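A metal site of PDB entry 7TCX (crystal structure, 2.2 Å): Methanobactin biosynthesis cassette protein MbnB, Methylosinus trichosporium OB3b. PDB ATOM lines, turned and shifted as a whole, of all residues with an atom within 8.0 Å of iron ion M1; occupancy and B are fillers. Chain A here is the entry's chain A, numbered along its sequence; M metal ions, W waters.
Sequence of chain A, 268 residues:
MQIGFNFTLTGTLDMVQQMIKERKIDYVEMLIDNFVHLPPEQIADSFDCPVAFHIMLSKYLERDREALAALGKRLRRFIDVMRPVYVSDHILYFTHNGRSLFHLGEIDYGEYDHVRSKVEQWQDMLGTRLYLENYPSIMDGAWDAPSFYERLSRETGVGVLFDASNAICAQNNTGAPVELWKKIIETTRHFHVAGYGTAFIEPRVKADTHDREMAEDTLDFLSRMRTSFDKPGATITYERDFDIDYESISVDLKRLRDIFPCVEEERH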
ATOM      1  N   HIS A  54     -23.558 -19.713  24.557  1.00  0.00           N
ATOM      2  CA  HIS A  54     -23.812 -18.380  24.011  1.00  0.00           C
ATOM      3  C   HIS A  54     -23.949 -18.538  22.504  1.00  0.00           C
ATOM      4  O   HIS A  54     -23.068 -19.100  21.859  1.00  0.00           O
ATOM      5  CB  HIS A  54     -22.660 -17.438  24.370  1.00  0.00           C
ATOM      6  CG  HIS A  54     -23.019 -15.983  24.341  1.00  0.00           C
ATOM      7  ND1 HIS A  54     -24.144 -15.462  24.945  1.00  0.00           N
ATOM      8  CD2 HIS A  54     -22.345 -14.923  23.825  1.00  0.00           C
ATOM      9  CE1 HIS A  54     -24.170 -14.156  24.765  1.00  0.00           C
ATOM     10  NE2 HIS A  54     -23.085 -13.808  24.097  1.00  0.00           N
ATOM     11  N   HIS A  90     -28.930 -13.228  21.570  1.00  0.00           N
ATOM     12  CA  HIS A  90     -28.784 -11.788  21.441  1.00  0.00           C
ATOM     13  C   HIS A  90     -30.052 -11.153  20.897  1.00  0.00           C
ATOM     14  O   HIS A  90     -30.936 -11.834  20.369  1.00  0.00           O
ATOM     15  CB  HIS A  90     -27.622 -11.432  20.512  1.00  0.00           C
ATOM     16  CG  HIS A  90     -26.285 -11.825  21.029  1.00  0.00           C
ATOM     17  ND1 HIS A  90     -25.783 -13.107  20.880  1.00  0.00           N
ATOM     18  CD2 HIS A  90     -25.335 -11.120  21.684  1.00  0.00           C
ATOM     19  CE1 HIS A  90     -24.581 -13.159  21.429  1.00  0.00           C
ATOM     20  NE2 HIS A  90     -24.287 -11.968  21.932  1.00  0.00           N
ATOM     21  N   GLU A 133     -29.158 -11.057  25.838  1.00  0.00           N
ATOM     22  CA  GLU A 133     -28.142 -10.127  26.301  1.00  0.00           C
ATOM     23  C   GLU A 133     -28.475  -8.699  25.871  1.00  0.00           C
ATOM     24  O   GLU A 133     -29.043  -8.470  24.805  1.00  0.00           O
ATOM     25  CB  GLU A 133     -26.785 -10.555  25.751  1.00  0.00           C
ATOM     26  CG  GLU A 133     -25.674  -9.529  25.906  1.00  0.00           C
ATOM     27  CD  GLU A 133     -24.318 -10.079  25.603  1.00  0.00           C
ATOM     28  OE1 GLU A 133     -24.216 -10.976  24.733  1.00  0.00           O
ATOM     29  OE2 GLU A 133     -23.343  -9.625  26.200  1.00  0.00           O
ATOM     30  N   ASN A 134     -28.117  -7.725  26.731  1.00  0.00           N
ATOM     31  CA  ASN A 134     -28.243  -6.300  26.381  1.00  0.00           C
ATOM     32  C   ASN A 134     -27.131  -5.854  25.420  1.00  0.00           C
ATOM     33  O   ASN A 134     -26.025  -6.373  25.438  1.00  0.00           O
ATOM     34  CB  ASN A 134     -28.178  -5.409  27.628  1.00  0.00           C
ATOM     35  CG  ASN A 134     -26.958  -5.712  28.491  1.00  0.00           C
ATOM     36  OD1 ASN A 134     -26.697  -6.887  28.850  1.00  0.00           O
ATOM     37  ND2 ASN A 134     -26.224  -4.659  28.851  1.00  0.00           N
ATOM     38  N   TYR A 135     -27.436  -4.828  24.633  1.00  0.00           N
ATOM     39  CA  TYR A 135     -26.612  -4.300  23.568  1.00  0.00           C
ATOM     40  C   TYR A 135     -25.757  -3.134  24.079  1.00  0.00           C
ATOM     41  O   TYR A 135     -26.219  -2.338  24.905  1.00  0.00           O
ATOM     42  CB  TYR A 135     -27.493  -3.838  22.400  1.00  0.00           C
ATOM     43  CG  TYR A 135     -26.727  -3.316  21.203  1.00  0.00           C
ATOM     44  CD1 TYR A 135     -26.270  -2.003  21.169  1.00  0.00           C
ATOM     45  CD2 TYR A 135     -26.469  -4.120  20.104  1.00  0.00           C
ATOM     46  CE1 TYR A 135     -25.548  -1.509  20.069  1.00  0.00           C
ATOM     47  CE2 TYR A 135     -25.755  -3.647  19.009  1.00  0.00           C
ATOM     48  CZ  TYR A 135     -25.298  -2.348  18.999  1.00  0.00           C
ATOM     49  OH  TYR A 135     -24.587  -1.896  17.892  1.00  0.00           O
ATOM     50  N   PRO A 136     -24.481  -3.026  23.644  1.00  0.00           N
ATOM     51  CA  PRO A 136     -23.615  -1.884  24.069  1.00  0.00           C
ATOM     52  C   PRO A 136     -23.918  -0.601  23.293  1.00  0.00           C
ATOM     53  O   PRO A 136     -23.197  -0.195  22.379  1.00  0.00           O
ATOM     54  CB  PRO A 136     -22.204  -2.404  23.751  1.00  0.00           C
ATOM     55  CG  PRO A 136     -22.427  -3.244  22.490  1.00  0.00           C
ATOM     56  CD  PRO A 136     -23.783  -3.904  22.694  1.00  0.00           C
ATOM     57  N   ASP A 163     -24.850  -7.940  30.583  1.00  0.00           N
ATOM     58  CA  ASP A 163     -23.453  -7.662  30.315  1.00  0.00           C
ATOM     59  C   ASP A 163     -23.143  -6.291  30.916  1.00  0.00           C
ATOM     60  O   ASP A 163     -23.586  -5.252  30.400  1.00  0.00           O
ATOM     61  CB  ASP A 163     -23.172  -7.703  28.820  1.00  0.00           C
ATOM     62  CG  ASP A 163     -21.695  -7.540  28.498  1.00  0.00           C
ATOM     63  OD1 ASP A 163     -21.076  -6.600  29.028  1.00  0.00           O
ATOM     64  OD2 ASP A 163     -21.146  -8.372  27.742  1.00  0.00           O
ATOM     65  N   ALA A 164     -22.370  -6.290  32.014  1.00  0.00           N
ATOM     66  CA  ALA A 164     -22.114  -5.053  32.751  1.00  0.00           C
ATOM     67  C   ALA A 164     -21.302  -4.050  31.922  1.00  0.00           C
ATOM     68  O   ALA A 164     -21.511  -2.834  32.006  1.00  0.00           O
ATOM     69  CB  ALA A 164     -21.376  -5.377  34.049  1.00  0.00           C
ATOM     70  N   SER A 165     -20.350  -4.537  31.125  1.00  0.00           N
ATOM     71  CA  SER A 165     -19.553  -3.551  30.408  1.00  0.00           C
ATOM     72  C   SER A 165     -20.301  -3.004  29.192  1.00  0.00           C
ATOM     73  O   SER A 165     -20.087  -1.839  28.833  1.00  0.00           O
ATOM     74  CB  SER A 165     -18.181  -4.140  30.028  1.00  0.00           C
ATOM     75  OG  SER A 165     -18.232  -5.360  29.310  1.00  0.00           O
ATOM     76  N   ASN A 166     -21.188  -3.786  28.560  1.00  0.00           N
ATOM     77  CA  ASN A 166     -22.037  -3.225  27.512  1.00  0.00           C
ATOM     78  C   ASN A 166     -22.890  -2.085  28.063  1.00  0.00           C
ATOM     79  O   ASN A 166     -23.124  -1.091  27.371  1.00  0.00           O
ATOM     80  CB  ASN A 166     -22.959  -4.266  26.907  1.00  0.00           C
ATOM     81  CG  ASN A 166     -22.223  -5.328  26.172  1.00  0.00           C
ATOM     82  OD1 ASN A 166     -20.998  -5.333  26.175  1.00  0.00           O
ATOM     83  ND2 ASN A 166     -22.950  -6.275  25.573  1.00  0.00           N
ATOM     84  N   ALA A 167     -23.380  -2.229  29.293  1.00  0.00           N
ATOM     85  CA  ALA A 167     -24.211  -1.189  29.886  1.00  0.00           C
ATOM     86  C   ALA A 167     -23.380   0.039  30.230  1.00  0.00           C
ATOM     87  O   ALA A 167     -23.856   1.176  30.098  1.00  0.00           O
ATOM     88  CB  ALA A 167     -24.926  -1.738  31.118  1.00  0.00           C
ATOM     89  N   CYS A 169     -20.732   0.879  28.469  1.00  0.00           N
ATOM     90  CA  CYS A 169     -20.629   1.498  27.156  1.00  0.00           C
ATOM     91  C   CYS A 169     -21.850   2.370  26.879  1.00  0.00           C
ATOM     92  O   CYS A 169     -21.725   3.535  26.486  1.00  0.00           O
ATOM     93  CB  CYS A 169     -20.499   0.443  26.055  1.00  0.00           C
ATOM     94  SG  CYS A 169     -18.872  -0.294  25.863  1.00  0.00           S
ATOM     95  N   HIS A 192     -22.170 -10.981  32.155  1.00  0.00           N
ATOM     96  CA  HIS A 192     -20.987 -10.809  31.326  1.00  0.00           C
ATOM     97  C   HIS A 192     -20.232  -9.564  31.767  1.00  0.00           C
ATOM     98  O   HIS A 192     -20.802  -8.615  32.305  1.00  0.00           O
ATOM     99  CB  HIS A 192     -21.330 -10.584  29.857  1.00  0.00           C
ATOM    100  CG  HIS A 192     -21.484 -11.825  29.055  1.00  0.00           C
ATOM    101  ND1 HIS A 192     -21.524 -11.812  27.683  1.00  0.00           N
ATOM    102  CD2 HIS A 192     -21.658 -13.114  29.427  1.00  0.00           C
ATOM    103  CE1 HIS A 192     -21.686 -13.043  27.241  1.00  0.00           C
ATOM    104  NE2 HIS A 192     -21.767 -13.849  28.274  1.00  0.00           N
ATOM    105  N   VAL A 193     -18.932  -9.568  31.472  1.00  0.00           N
ATOM    106  CA  VAL A 193     -18.119  -8.371  31.612  1.00  0.00           C
ATOM    107  C   VAL A 193     -16.890  -8.546  30.732  1.00  0.00           C
ATOM    108  O   VAL A 193     -16.442  -9.682  30.493  1.00  0.00           O
ATOM    109  CB  VAL A 193     -17.753  -8.122  33.099  1.00  0.00           C
ATOM    110  CG1 VAL A 193     -16.740  -9.146  33.581  1.00  0.00           C
ATOM    111  CG2 VAL A 193     -17.215  -6.721  33.260  1.00  0.00           C
ATOM    112  N   ALA A 194     -16.374  -7.429  30.212  1.00  0.00           N
ATOM    113  CA  ALA A 194     -15.209  -7.427  29.339  1.00  0.00           C
ATOM    114  C   ALA A 194     -14.610  -6.022  29.301  1.00  0.00           C
ATOM    115  O   ALA A 194     -15.149  -5.075  29.879  1.00  0.00           O
ATOM    116  CB  ALA A 194     -15.564  -7.896  27.933  1.00  0.00           C
ATOM    117  N   GLY A 195     -13.466  -5.907  28.627  1.00  0.00           N
ATOM    118  CA  GLY A 195     -12.916  -4.602  28.331  1.00  0.00           C
ATOM    119  C   GLY A 195     -13.573  -4.015  27.098  1.00  0.00           C
ATOM    120  O   GLY A 195     -14.113  -4.715  26.241  1.00  0.00           O
ATOM    121  N   TYR A 196     -13.559  -2.696  27.014  1.00  0.00           N
ATOM    122  CA  TYR A 196     -14.059  -2.015  25.842  1.00  0.00           C
ATOM    123  C   TYR A 196     -13.025  -1.004  25.334  1.00  0.00           C
ATOM    124  O   TYR A 196     -12.199  -0.490  26.101  1.00  0.00           O
ATOM    125  CB  TYR A 196     -15.397  -1.325  26.125  1.00  0.00           C
ATOM    126  CG  TYR A 196     -15.355  -0.315  27.243  1.00  0.00           C
ATOM    127  CD1 TYR A 196     -14.816   0.950  27.055  1.00  0.00           C
ATOM    128  CD2 TYR A 196     -15.884  -0.625  28.495  1.00  0.00           C
ATOM    129  CE1 TYR A 196     -14.778   1.866  28.058  1.00  0.00           C
ATOM    130  CE2 TYR A 196     -15.851   0.278  29.514  1.00  0.00           C
ATOM    131  CZ  TYR A 196     -15.304   1.527  29.293  1.00  0.00           C
ATOM    132  OH  TYR A 196     -15.287   2.445  30.313  1.00  0.00           O
ATOM    133  N   ALA A 207     -16.534   1.475  22.188  1.00  0.00           N
ATOM    134  CA  ALA A 207     -16.770   0.326  21.314  1.00  0.00           C
ATOM    135  C   ALA A 207     -16.561  -0.962  22.086  1.00  0.00           C
ATOM    136  O   ALA A 207     -15.579  -1.103  22.826  1.00  0.00           O
ATOM    137  CB  ALA A 207     -15.815   0.347  20.110  1.00  0.00           C
ATOM    138  N   ASP A 208     -17.482  -1.923  21.889  1.00  0.00           N
ATOM    139  CA  ASP A 208     -17.530  -3.179  22.659  1.00  0.00           C
ATOM    140  C   ASP A 208     -16.644  -4.225  21.999  1.00  0.00           C
ATOM    141  O   ASP A 208     -17.098  -5.108  21.268  1.00  0.00           O
ATOM    142  CB  ASP A 208     -18.972  -3.662  22.774  1.00  0.00           C
ATOM    143  CG  ASP A 208     -19.131  -4.788  23.800  1.00  0.00           C
ATOM    144  OD1 ASP A 208     -18.615  -4.640  24.927  1.00  0.00           O
ATOM    145  OD2 ASP A 208     -19.774  -5.821  23.461  1.00  0.00           O
ATOM    146  N   THR A 209     -15.347  -4.144  22.291  1.00  0.00           N
ATOM    147  CA  THR A 209     -14.314  -4.830  21.523  1.00  0.00           C
ATOM    148  C   THR A 209     -13.764  -6.089  22.185  1.00  0.00           C
ATOM    149  O   THR A 209     -13.196  -6.928  21.490  1.00  0.00           O
ATOM    150  CB  THR A 209     -13.158  -3.861  21.236  1.00  0.00           C
ATOM    151  OG1 THR A 209     -12.671  -3.338  22.479  1.00  0.00           O
ATOM    152  CG2 THR A 209     -13.656  -2.697  20.377  1.00  0.00           C
ATOM    153  N   HIS A 210     -13.917  -6.220  23.523  1.00  0.00           N
ATOM    154  CA  HIS A 210     -13.473  -7.410  24.271  1.00  0.00           C
ATOM    155  C   HIS A 210     -12.010  -7.728  24.024  1.00  0.00           C
ATOM    156  O   HIS A 210     -11.624  -8.877  23.858  1.00  0.00           O
ATOM    157  CB  HIS A 210     -14.305  -8.653  23.928  1.00  0.00           C
ATOM    158  CG  HIS A 210     -15.770  -8.451  24.095  1.00  0.00           C
ATOM    159  ND1 HIS A 210     -16.686  -9.409  23.730  1.00  0.00           N
ATOM    160  CD2 HIS A 210     -16.478  -7.419  24.605  1.00  0.00           C
ATOM    161  CE1 HIS A 210     -17.904  -8.966  23.984  1.00  0.00           C
ATOM    162  NE2 HIS A 210     -17.804  -7.755  24.511  1.00  0.00           N
ATOM    163  N   GLU A 239     -15.151 -11.895  29.069  1.00  0.00           N
ATOM    164  CA  GLU A 239     -15.036 -12.054  27.620  1.00  0.00           C
ATOM    165  C   GLU A 239     -13.716 -11.461  27.137  1.00  0.00           C
ATOM    166  O   GLU A 239     -13.399 -10.311  27.456  1.00  0.00           O
ATOM    167  CB  GLU A 239     -16.193 -11.392  26.890  1.00  0.00           C
ATOM    168  CG  GLU A 239     -17.554 -11.767  27.428  1.00  0.00           C
ATOM    169  CD  GLU A 239     -18.676 -11.232  26.564  1.00  0.00           C
ATOM    170  OE1 GLU A 239     -18.988 -11.824  25.511  1.00  0.00           O
ATOM    171  OE2 GLU A 239     -19.243 -10.187  26.953  1.00  0.00           O
ATOM    172  N   ASP A 241     -11.984 -11.563  23.318  1.00  0.00           N
ATOM    173  CA  ASP A 241     -12.091 -12.069  21.959  1.00  0.00           C
ATOM    174  C   ASP A 241     -10.877 -11.744  21.102  1.00  0.00           C
ATOM    175  O   ASP A 241     -10.674 -12.371  20.067  1.00  0.00           O
ATOM    176  CB  ASP A 241     -13.360 -11.515  21.298  1.00  0.00           C
ATOM    177  CG  ASP A 241     -14.646 -12.021  21.974  1.00  0.00           C
ATOM    178  OD1 ASP A 241     -14.657 -13.174  22.455  1.00  0.00           O
ATOM    179  OD2 ASP A 241     -15.646 -11.284  22.036  1.00  0.00           O
HETATM  180 FE    FE M   1     -19.673  -6.879  25.390  1.00  0.00          FE
HETATM  181 FE    FE M   2     -21.302  -9.877  26.294  1.00  0.00          FE
HETATM  182 FE    FE M   3     -22.699 -11.668  23.339  1.00  0.00          FE
HETATM  183  O   HOH W   1     -18.793  -7.145  27.302  1.00  0.00           O
HETATM  184  O   HOH W   2     -21.078  -8.359  24.403  1.00  0.00           O
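Asp 163 touches iron ion M1 (OD2 to FE, 3.2 Å).
OE2 of Glu 239 touches iron ion M1 (3.7 Å).
Of the 23 residues printed, 5 come within 4 Å of iron ion M1.
Water W1 bridges the side-chain hydroxyl of Ser 165 (2.7 Å) and the side-chain carboxylate of Asp 163 (2.9 Å).
Iron ion M1 is bound by water W1 (2.1 Å), the side-chain amide oxygen (OD1) of Asn 166 (2.2 Å), the side-chain carboxylate (OD2) of Asp 208 (2.2 Å), a ring nitrogen (NE2) of His 210 (2.2 Å), water W2 (2.3 Å) and the side-chain carboxylate (OD1) of Asp 208 (2.5 Å).
Iron ion M1 has six donor atoms within binding distance.
The backbone NH (N) of Asp 163 is in hydrogen-bond range of the side-chain amide oxygen (OD1) of Asn 134 (2.7 Å).
N of His 210 is in hydrogen-bond range of O of Gly 195 (3.1 Å).
The side-chain amide nitrogen (ND2) of Asn 166 sits at hydrogen-bond distance from the backbone carbonyl oxygen (O) of Asn 134 (3.1 Å).
ND2 of Asn 166 sits close to OE2 of Glu 133 (3.4 Å).
A ring nitrogen (ND1) of His 210 is in hydrogen-bond range of the side-chain carboxylate of Asp 241, 2.7 Å away.
O of Val 193 is in hydrogen-bond range of N of Glu 239, at 2.9 Å.
The backbone NH of Ser 165 is in hydrogen-bond range of the side-chain carboxylate of Asp 163 (3.0 Å).
N of Asn 166 sits at hydrogen-bond distance from OD1 of Asp 163.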
